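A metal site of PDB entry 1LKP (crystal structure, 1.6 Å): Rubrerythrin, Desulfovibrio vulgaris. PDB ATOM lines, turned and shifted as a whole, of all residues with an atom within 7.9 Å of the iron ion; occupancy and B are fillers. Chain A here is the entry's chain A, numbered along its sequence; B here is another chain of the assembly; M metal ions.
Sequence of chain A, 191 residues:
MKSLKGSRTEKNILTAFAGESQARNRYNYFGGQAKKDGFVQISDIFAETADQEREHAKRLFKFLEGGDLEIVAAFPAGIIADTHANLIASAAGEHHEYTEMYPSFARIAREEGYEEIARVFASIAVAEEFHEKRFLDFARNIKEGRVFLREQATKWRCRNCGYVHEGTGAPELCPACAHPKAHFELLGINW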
ATOM      1  N   ARG A 157     -17.907  21.278 -19.723  1.00  0.00           N
ATOM      2  CA  ARG A 157     -17.250  20.324 -20.617  1.00  0.00           C
ATOM      3  C   ARG A 157     -15.811  20.083 -20.190  1.00  0.00           C
ATOM      4  O   ARG A 157     -15.088  21.009 -19.828  1.00  0.00           O
ATOM      5  CB  ARG A 157     -17.258  20.845 -22.060  1.00  0.00           C
ATOM      6  CG  ARG A 157     -16.771  19.805 -23.080  1.00  0.00           C
ATOM      7  CD  ARG A 157     -16.635  20.391 -24.490  1.00  0.00           C
ATOM      8  NE  ARG A 157     -15.494  21.309 -24.603  1.00  0.00           N
ATOM      9  CZ  ARG A 157     -14.509  21.165 -25.482  1.00  0.00           C
ATOM     10  NH1 ARG A 157     -14.508  20.142 -26.323  1.00  0.00           N
ATOM     11  NH2 ARG A 157     -13.519  22.053 -25.518  1.00  0.00           N
ATOM     12  N   CYS A 158     -15.395  18.816 -20.217  1.00  0.00           N
ATOM     13  CA  CYS A 158     -14.028  18.461 -19.862  1.00  0.00           C
ATOM     14  C   CYS A 158     -13.196  18.692 -21.127  1.00  0.00           C
ATOM     15  O   CYS A 158     -13.428  18.044 -22.149  1.00  0.00           O
ATOM     16  CB  CYS A 158     -13.940  16.991 -19.451  1.00  0.00           C
ATOM     17  SG  CYS A 158     -12.250  16.408 -19.208  1.00  0.00           S
ATOM     18  N   ARG A 159     -12.241  19.605 -21.062  1.00  0.00           N
ATOM     19  CA  ARG A 159     -11.410  19.870 -22.239  1.00  0.00           C
ATOM     20  C   ARG A 159     -10.540  18.676 -22.619  1.00  0.00           C
ATOM     21  O   ARG A 159     -10.168  18.515 -23.779  1.00  0.00           O
ATOM     22  CB  ARG A 159     -10.525  21.112 -21.997  1.00  0.00           C
ATOM     23  CG  ARG A 159     -11.300  22.429 -21.997  1.00  0.00           C
ATOM     24  CD  ARG A 159     -10.367  23.637 -21.828  1.00  0.00           C
ATOM     25  NE  ARG A 159      -9.434  23.774 -22.948  1.00  0.00           N
ATOM     26  CZ  ARG A 159      -9.773  24.163 -24.177  1.00  0.00           C
ATOM     27  NH1 ARG A 159     -11.035  24.476 -24.472  1.00  0.00           N
ATOM     28  NH2 ARG A 159      -8.842  24.237 -25.124  1.00  0.00           N
ATOM     29  N   ASN A 160     -10.226  17.822 -21.651  1.00  0.00           N
ATOM     30  CA  ASN A 160      -9.376  16.657 -21.921  1.00  0.00           C
ATOM     31  C   ASN A 160     -10.057  15.545 -22.730  1.00  0.00           C
ATOM     32  O   ASN A 160      -9.429  14.979 -23.645  1.00  0.00           O
ATOM     33  CB  ASN A 160      -8.847  16.055 -20.620  1.00  0.00           C
ATOM     34  CG  ASN A 160      -7.797  14.984 -20.848  1.00  0.00           C
ATOM     35  OD1 ASN A 160      -8.001  13.806 -20.523  1.00  0.00           O
ATOM     36  ND2 ASN A 160      -6.664  15.387 -21.417  1.00  0.00           N
ATOM     37  N   CYS A 161     -11.309  15.246 -22.425  1.00  0.00           N
ATOM     38  CA  CYS A 161     -12.010  14.163 -23.124  1.00  0.00           C
ATOM     39  C   CYS A 161     -13.390  14.482 -23.688  1.00  0.00           C
ATOM     40  O   CYS A 161     -13.992  13.649 -24.357  1.00  0.00           O
ATOM     41  CB  CYS A 161     -12.141  12.950 -22.201  1.00  0.00           C
ATOM     42  SG  CYS A 161     -13.427  13.137 -20.928  1.00  0.00           S
ATOM     43  N   GLY A 162     -13.894  15.682 -23.416  1.00  0.00           N
ATOM     44  CA  GLY A 162     -15.196  16.041 -23.953  1.00  0.00           C
ATOM     45  C   GLY A 162     -16.412  15.676 -23.111  1.00  0.00           C
ATOM     46  O   GLY A 162     -17.539  15.922 -23.527  1.00  0.00           O
ATOM     47  N   TYR A 163     -16.202  15.066 -21.955  1.00  0.00           N
ATOM     48  CA  TYR A 163     -17.325  14.702 -21.094  1.00  0.00           C
ATOM     49  C   TYR A 163     -18.118  15.965 -20.744  1.00  0.00           C
ATOM     50  O   TYR A 163     -17.545  17.029 -20.532  1.00  0.00           O
ATOM     51  CB  TYR A 163     -16.835  14.042 -19.809  1.00  0.00           C
ATOM     52  CG  TYR A 163     -17.953  13.698 -18.854  1.00  0.00           C
ATOM     53  CD1 TYR A 163     -18.801  12.627 -19.102  1.00  0.00           C
ATOM     54  CD2 TYR A 163     -18.192  14.485 -17.725  1.00  0.00           C
ATOM     55  CE1 TYR A 163     -19.871  12.339 -18.246  1.00  0.00           C
ATOM     56  CE2 TYR A 163     -19.265  14.221 -16.875  1.00  0.00           C
ATOM     57  CZ  TYR A 163     -20.096  13.144 -17.137  1.00  0.00           C
ATOM     58  OH  TYR A 163     -21.146  12.860 -16.293  1.00  0.00           O
ATOM     59  N   VAL A 164     -19.437  15.833 -20.677  1.00  0.00           N
ATOM     60  CA  VAL A 164     -20.288  16.958 -20.332  1.00  0.00           C
ATOM     61  C   VAL A 164     -20.951  16.677 -18.996  1.00  0.00           C
ATOM     62  O   VAL A 164     -21.610  15.638 -18.813  1.00  0.00           O
ATOM     63  CB  VAL A 164     -21.381  17.176 -21.401  1.00  0.00           C
ATOM     64  CG1 VAL A 164     -22.294  18.330 -20.982  1.00  0.00           C
ATOM     65  CG2 VAL A 164     -20.730  17.484 -22.742  1.00  0.00           C
ATOM     66  N   LEU A 173     -13.333  15.385 -10.211  1.00  0.00           N
ATOM     67  CA  LEU A 173     -12.662  14.484 -11.148  1.00  0.00           C
ATOM     68  C   LEU A 173     -13.624  14.148 -12.279  1.00  0.00           C
ATOM     69  O   LEU A 173     -14.813  13.928 -12.040  1.00  0.00           O
ATOM     70  CB  LEU A 173     -12.245  13.189 -10.454  1.00  0.00           C
ATOM     71  CG  LEU A 173     -11.081  13.255  -9.458  1.00  0.00           C
ATOM     72  CD1 LEU A 173     -10.854  11.868  -8.856  1.00  0.00           C
ATOM     73  CD2 LEU A 173      -9.812  13.735 -10.163  1.00  0.00           C
ATOM     74  N   CYS A 174     -13.121  14.123 -13.504  1.00  0.00           N
ATOM     75  CA  CYS A 174     -13.959  13.799 -14.648  1.00  0.00           C
ATOM     76  C   CYS A 174     -14.318  12.310 -14.561  1.00  0.00           C
ATOM     77  O   CYS A 174     -13.449  11.454 -14.443  1.00  0.00           O
ATOM     78  CB  CYS A 174     -13.206  14.070 -15.957  1.00  0.00           C
ATOM     79  SG  CYS A 174     -14.155  13.613 -17.427  1.00  0.00           S
ATOM     80  N   PRO A 175     -15.618  11.985 -14.602  1.00  0.00           N
ATOM     81  CA  PRO A 175     -16.001  10.573 -14.520  1.00  0.00           C
ATOM     82  C   PRO A 175     -15.580   9.725 -15.712  1.00  0.00           C
ATOM     83  O   PRO A 175     -15.569   8.491 -15.630  1.00  0.00           O
ATOM     84  CB  PRO A 175     -17.515  10.635 -14.343  1.00  0.00           C
ATOM     85  CG  PRO A 175     -17.881  11.872 -15.106  1.00  0.00           C
ATOM     86  CD  PRO A 175     -16.803  12.854 -14.678  1.00  0.00           C
ATOM     87  N   ALA A 176     -15.237  10.372 -16.822  1.00  0.00           N
ATOM     88  CA  ALA A 176     -14.807   9.651 -18.014  1.00  0.00           C
ATOM     89  C   ALA A 176     -13.291   9.432 -18.075  1.00  0.00           C
ATOM     90  O   ALA A 176     -12.838   8.294 -18.125  1.00  0.00           O
ATOM     91  CB  ALA A 176     -15.265  10.403 -19.268  1.00  0.00           C
ATOM     92  N   CYS A 177     -12.519  10.506 -18.041  1.00  0.00           N
ATOM     93  CA  CYS A 177     -11.064  10.394 -18.136  1.00  0.00           C
ATOM     94  C   CYS A 177     -10.282  10.504 -16.827  1.00  0.00           C
ATOM     95  O   CYS A 177      -9.047  10.402 -16.831  1.00  0.00           O
ATOM     96  CB  CYS A 177     -10.527  11.427 -19.133  1.00  0.00           C
ATOM     97  SG  CYS A 177     -10.555  13.124 -18.509  1.00  0.00           S
ATOM     98  N   ALA A 178     -10.981  10.728 -15.726  1.00  0.00           N
ATOM     99  CA  ALA A 178     -10.350  10.837 -14.408  1.00  0.00           C
ATOM    100  C   ALA A 178      -9.412  12.016 -14.204  1.00  0.00           C
ATOM    101  O   ALA A 178      -8.654  12.044 -13.234  1.00  0.00           O
ATOM    102  CB  ALA A 178      -9.627   9.526 -14.073  1.00  0.00           C
ATOM    103  N   HIS A 179      -9.425  12.984 -15.120  1.00  0.00           N
ATOM    104  CA  HIS A 179      -8.566  14.147 -14.949  1.00  0.00           C
ATOM    105  C   HIS A 179      -9.242  15.121 -13.968  1.00  0.00           C
ATOM    106  O   HIS A 179     -10.456  15.085 -13.796  1.00  0.00           O
ATOM    107  CB  HIS A 179      -8.273  14.809 -16.285  1.00  0.00           C
ATOM    108  CG  HIS A 179      -7.219  14.097 -17.076  1.00  0.00           C
ATOM    109  ND1 HIS A 179      -7.274  12.748 -17.352  1.00  0.00           N
ATOM    110  CD2 HIS A 179      -6.064  14.543 -17.619  1.00  0.00           C
ATOM    111  CE1 HIS A 179      -6.201  12.399 -18.032  1.00  0.00           C
ATOM    112  NE2 HIS A 179      -5.442  13.459 -18.204  1.00  0.00           N
ATOM    113  N   PRO A 180      -8.453  15.983 -13.308  1.00  0.00           N
ATOM    114  CA  PRO A 180      -8.998  16.935 -12.347  1.00  0.00           C
ATOM    115  C   PRO A 180      -9.885  18.055 -12.878  1.00  0.00           C
ATOM    116  O   PRO A 180      -9.884  18.369 -14.072  1.00  0.00           O
ATOM    117  CB  PRO A 180      -7.756  17.462 -11.640  1.00  0.00           C
ATOM    118  CG  PRO A 180      -6.724  17.418 -12.712  1.00  0.00           C
ATOM    119  CD  PRO A 180      -6.981  16.093 -13.387  1.00  0.00           C
ATOM    120  N   HIS A 183      -9.549  20.789 -15.765  1.00  0.00           N
ATOM    121  CA  HIS A 183      -9.807  20.650 -17.198  1.00  0.00           C
ATOM    122  C   HIS A 183     -11.186  21.111 -17.666  1.00  0.00           C
ATOM    123  O   HIS A 183     -11.444  21.177 -18.869  1.00  0.00           O
ATOM    124  CB  HIS A 183      -9.579  19.204 -17.620  1.00  0.00           C
ATOM    125  CG  HIS A 183      -8.142  18.771 -17.522  1.00  0.00           C
ATOM    126  ND1 HIS A 183      -7.279  18.823 -18.597  1.00  0.00           N
ATOM    127  CD2 HIS A 183      -7.411  18.351 -16.472  1.00  0.00           C
ATOM    128  CE1 HIS A 183      -6.078  18.449 -18.203  1.00  0.00           C
ATOM    129  NE2 HIS A 183      -6.128  18.157 -16.917  1.00  0.00           N
ATOM    130  N   PHE A 184     -12.073  21.436 -16.728  1.00  0.00           N
ATOM    131  CA  PHE A 184     -13.424  21.842 -17.107  1.00  0.00           C
ATOM    132  C   PHE A 184     -13.632  23.314 -17.461  1.00  0.00           C
ATOM    133  O   PHE A 184     -12.950  24.208 -16.955  1.00  0.00           O
ATOM    134  CB  PHE A 184     -14.419  21.440 -16.024  1.00  0.00           C
ATOM    135  CG  PHE A 184     -14.718  19.965 -15.994  1.00  0.00           C
ATOM    136  CD1 PHE A 184     -13.873  19.078 -15.326  1.00  0.00           C
ATOM    137  CD2 PHE A 184     -15.835  19.456 -16.663  1.00  0.00           C
ATOM    138  CE1 PHE A 184     -14.125  17.707 -15.335  1.00  0.00           C
ATOM    139  CE2 PHE A 184     -16.093  18.078 -16.683  1.00  0.00           C
ATOM    140  CZ  PHE A 184     -15.240  17.209 -16.013  1.00  0.00           C
ATOM    141  N   GLN B  52      -9.291  14.039 -27.917  1.00  0.00           N
ATOM    142  CA  GLN B  52     -10.152  13.548 -26.856  1.00  0.00           C
ATOM    143  C   GLN B  52     -10.356  12.039 -26.998  1.00  0.00           C
ATOM    144  O   GLN B  52     -10.464  11.344 -25.988  1.00  0.00           O
ATOM    145  CB  GLN B  52     -11.470  14.323 -26.849  1.00  0.00           C
ATOM    146  CG  GLN B  52     -11.228  15.811 -26.583  1.00  0.00           C
ATOM    147  CD  GLN B  52     -12.473  16.651 -26.461  1.00  0.00           C
ATOM    148  OE1 GLN B  52     -13.498  16.358 -27.064  1.00  0.00           O
ATOM    149  NE2 GLN B  52     -12.383  17.742 -25.692  1.00  0.00           N
ATOM    150  N   GLU B  55      -7.691  10.339 -25.344  1.00  0.00           N
ATOM    151  CA  GLU B  55      -7.887  10.280 -23.897  1.00  0.00           C
ATOM    152  C   GLU B  55      -8.885   9.188 -23.485  1.00  0.00           C
ATOM    153  O   GLU B  55      -8.746   8.588 -22.430  1.00  0.00           O
ATOM    154  CB  GLU B  55      -8.290  11.647 -23.364  1.00  0.00           C
ATOM    155  CG  GLU B  55      -7.187  12.701 -23.561  1.00  0.00           C
ATOM    156  CD  GLU B  55      -5.884  12.324 -22.874  1.00  0.00           C
ATOM    157  OE1 GLU B  55      -5.919  11.907 -21.693  1.00  0.00           O
ATOM    158  OE2 GLU B  55      -4.798  12.459 -23.503  1.00  0.00           O
ATOM    159  N   HIS B  56      -9.908   8.951 -24.304  1.00  0.00           N
ATOM    160  CA  HIS B  56     -10.852   7.880 -23.988  1.00  0.00           C
ATOM    161  C   HIS B  56     -10.050   6.579 -24.049  1.00  0.00           C
ATOM    162  O   HIS B  56     -10.167   5.718 -23.180  1.00  0.00           O
ATOM    163  CB  HIS B  56     -11.971   7.788 -25.035  1.00  0.00           C
ATOM    164  CG  HIS B  56     -12.863   8.976 -25.083  1.00  0.00           C
ATOM    165  ND1 HIS B  56     -13.777   9.176 -26.096  1.00  0.00           N
ATOM    166  CD2 HIS B  56     -12.978  10.052 -24.259  1.00  0.00           C
ATOM    167  CE1 HIS B  56     -14.417  10.323 -25.898  1.00  0.00           C
ATOM    168  NE2 HIS B  56     -13.946  10.867 -24.791  1.00  0.00           N
ATOM    169  N   ARG B  59      -7.731   5.989 -20.994  1.00  0.00           N
ATOM    170  CA  ARG B  59      -8.445   5.550 -19.801  1.00  0.00           C
ATOM    171  C   ARG B  59      -8.737   4.055 -19.918  1.00  0.00           C
ATOM    172  O   ARG B  59      -8.541   3.300 -18.969  1.00  0.00           O
ATOM    173  CB  ARG B  59      -9.767   6.320 -19.640  1.00  0.00           C
ATOM    174  CG  ARG B  59     -10.530   5.979 -18.352  1.00  0.00           C
ATOM    175  CD  ARG B  59      -9.799   6.505 -17.118  1.00  0.00           C
ATOM    176  NE  ARG B  59     -10.232   5.892 -15.868  1.00  0.00           N
ATOM    177  CZ  ARG B  59     -11.285   6.270 -15.145  1.00  0.00           C
ATOM    178  NH1 ARG B  59     -12.047   7.276 -15.538  1.00  0.00           N
ATOM    179  NH2 ARG B  59     -11.559   5.644 -14.010  1.00  0.00           N
ATOM    180  N   SER B 123     -19.867   7.157 -19.128  1.00  0.00           N
ATOM    181  CA  SER B 123     -19.371   8.523 -19.152  1.00  0.00           C
ATOM    182  C   SER B 123     -18.769   8.877 -20.509  1.00  0.00           C
ATOM    183  O   SER B 123     -18.970   9.969 -21.021  1.00  0.00           O
ATOM    184  CB  SER B 123     -18.338   8.722 -18.044  1.00  0.00           C
ATOM    185  OG  SER B 123     -18.959   8.573 -16.772  1.00  0.00           O
ATOM    186  N   ALA B 127     -19.615  11.906 -23.744  1.00  0.00           N
ATOM    187  CA  ALA B 127     -18.678  12.696 -24.548  1.00  0.00           C
ATOM    188  C   ALA B 127     -18.950  12.493 -26.031  1.00  0.00           C
ATOM    189  O   ALA B 127     -18.969  13.457 -26.804  1.00  0.00           O
ATOM    190  CB  ALA B 127     -17.244  12.283 -24.232  1.00  0.00           C
HETATM  191 FE    FE M   1     -12.607  14.099 -19.058  1.00  0.00          FE
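The iron ion is bound by the side-chain sulfur of Cys 161, the side-chain sulfur of Cys 174, the side-chain sulfur of Cys 177 and the side-chain sulfur of Cys 158.
The iron ion has four donor atoms within binding distance.
The side-chain sulfur of Cys 161 sits close to the backbone NH of Tyr 163 (3.5 Å).
The backbone carbonyl oxygen (O) of Cys 161 sits at hydrogen-bond distance from a ring nitrogen (NE2) of His 56 of chain B (2.8 Å).
The side-chain sulfur (SG) of Cys 174 lies close to the backbone NH (N) of Ala 176 (3.5 Å).
N of Cys 174 lies within hydrogen-bond range of O of His 179 (2.8 Å).
The side-chain amide oxygen (OD1) of Asn 160 sits close to the side-chain sulfur (SG) of Cys 177 (3.3 Å).
A ring nitrogen (ND1) of His 179 is in hydrogen-bond range of the backbone carbonyl oxygen (O) of Cys 177 (3.0 Å).
The backbone NH of Cys 158 sits at hydrogen-bond distance from the backbone carbonyl oxygen of Tyr 163, at 2.8 Å.
SG of Cys 158 lies close to N of Asn 160.
Four residues have an atom within 4 Å of the iron ion: Cys 158, Cys 161, Cys 174 and Cys 177.
Along chain A the residues within 4 Å of the iron ion span positions 158 to 177.
The nearest printed residue that does not touch the iron ion is Tyr 163 (4.3 Å).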
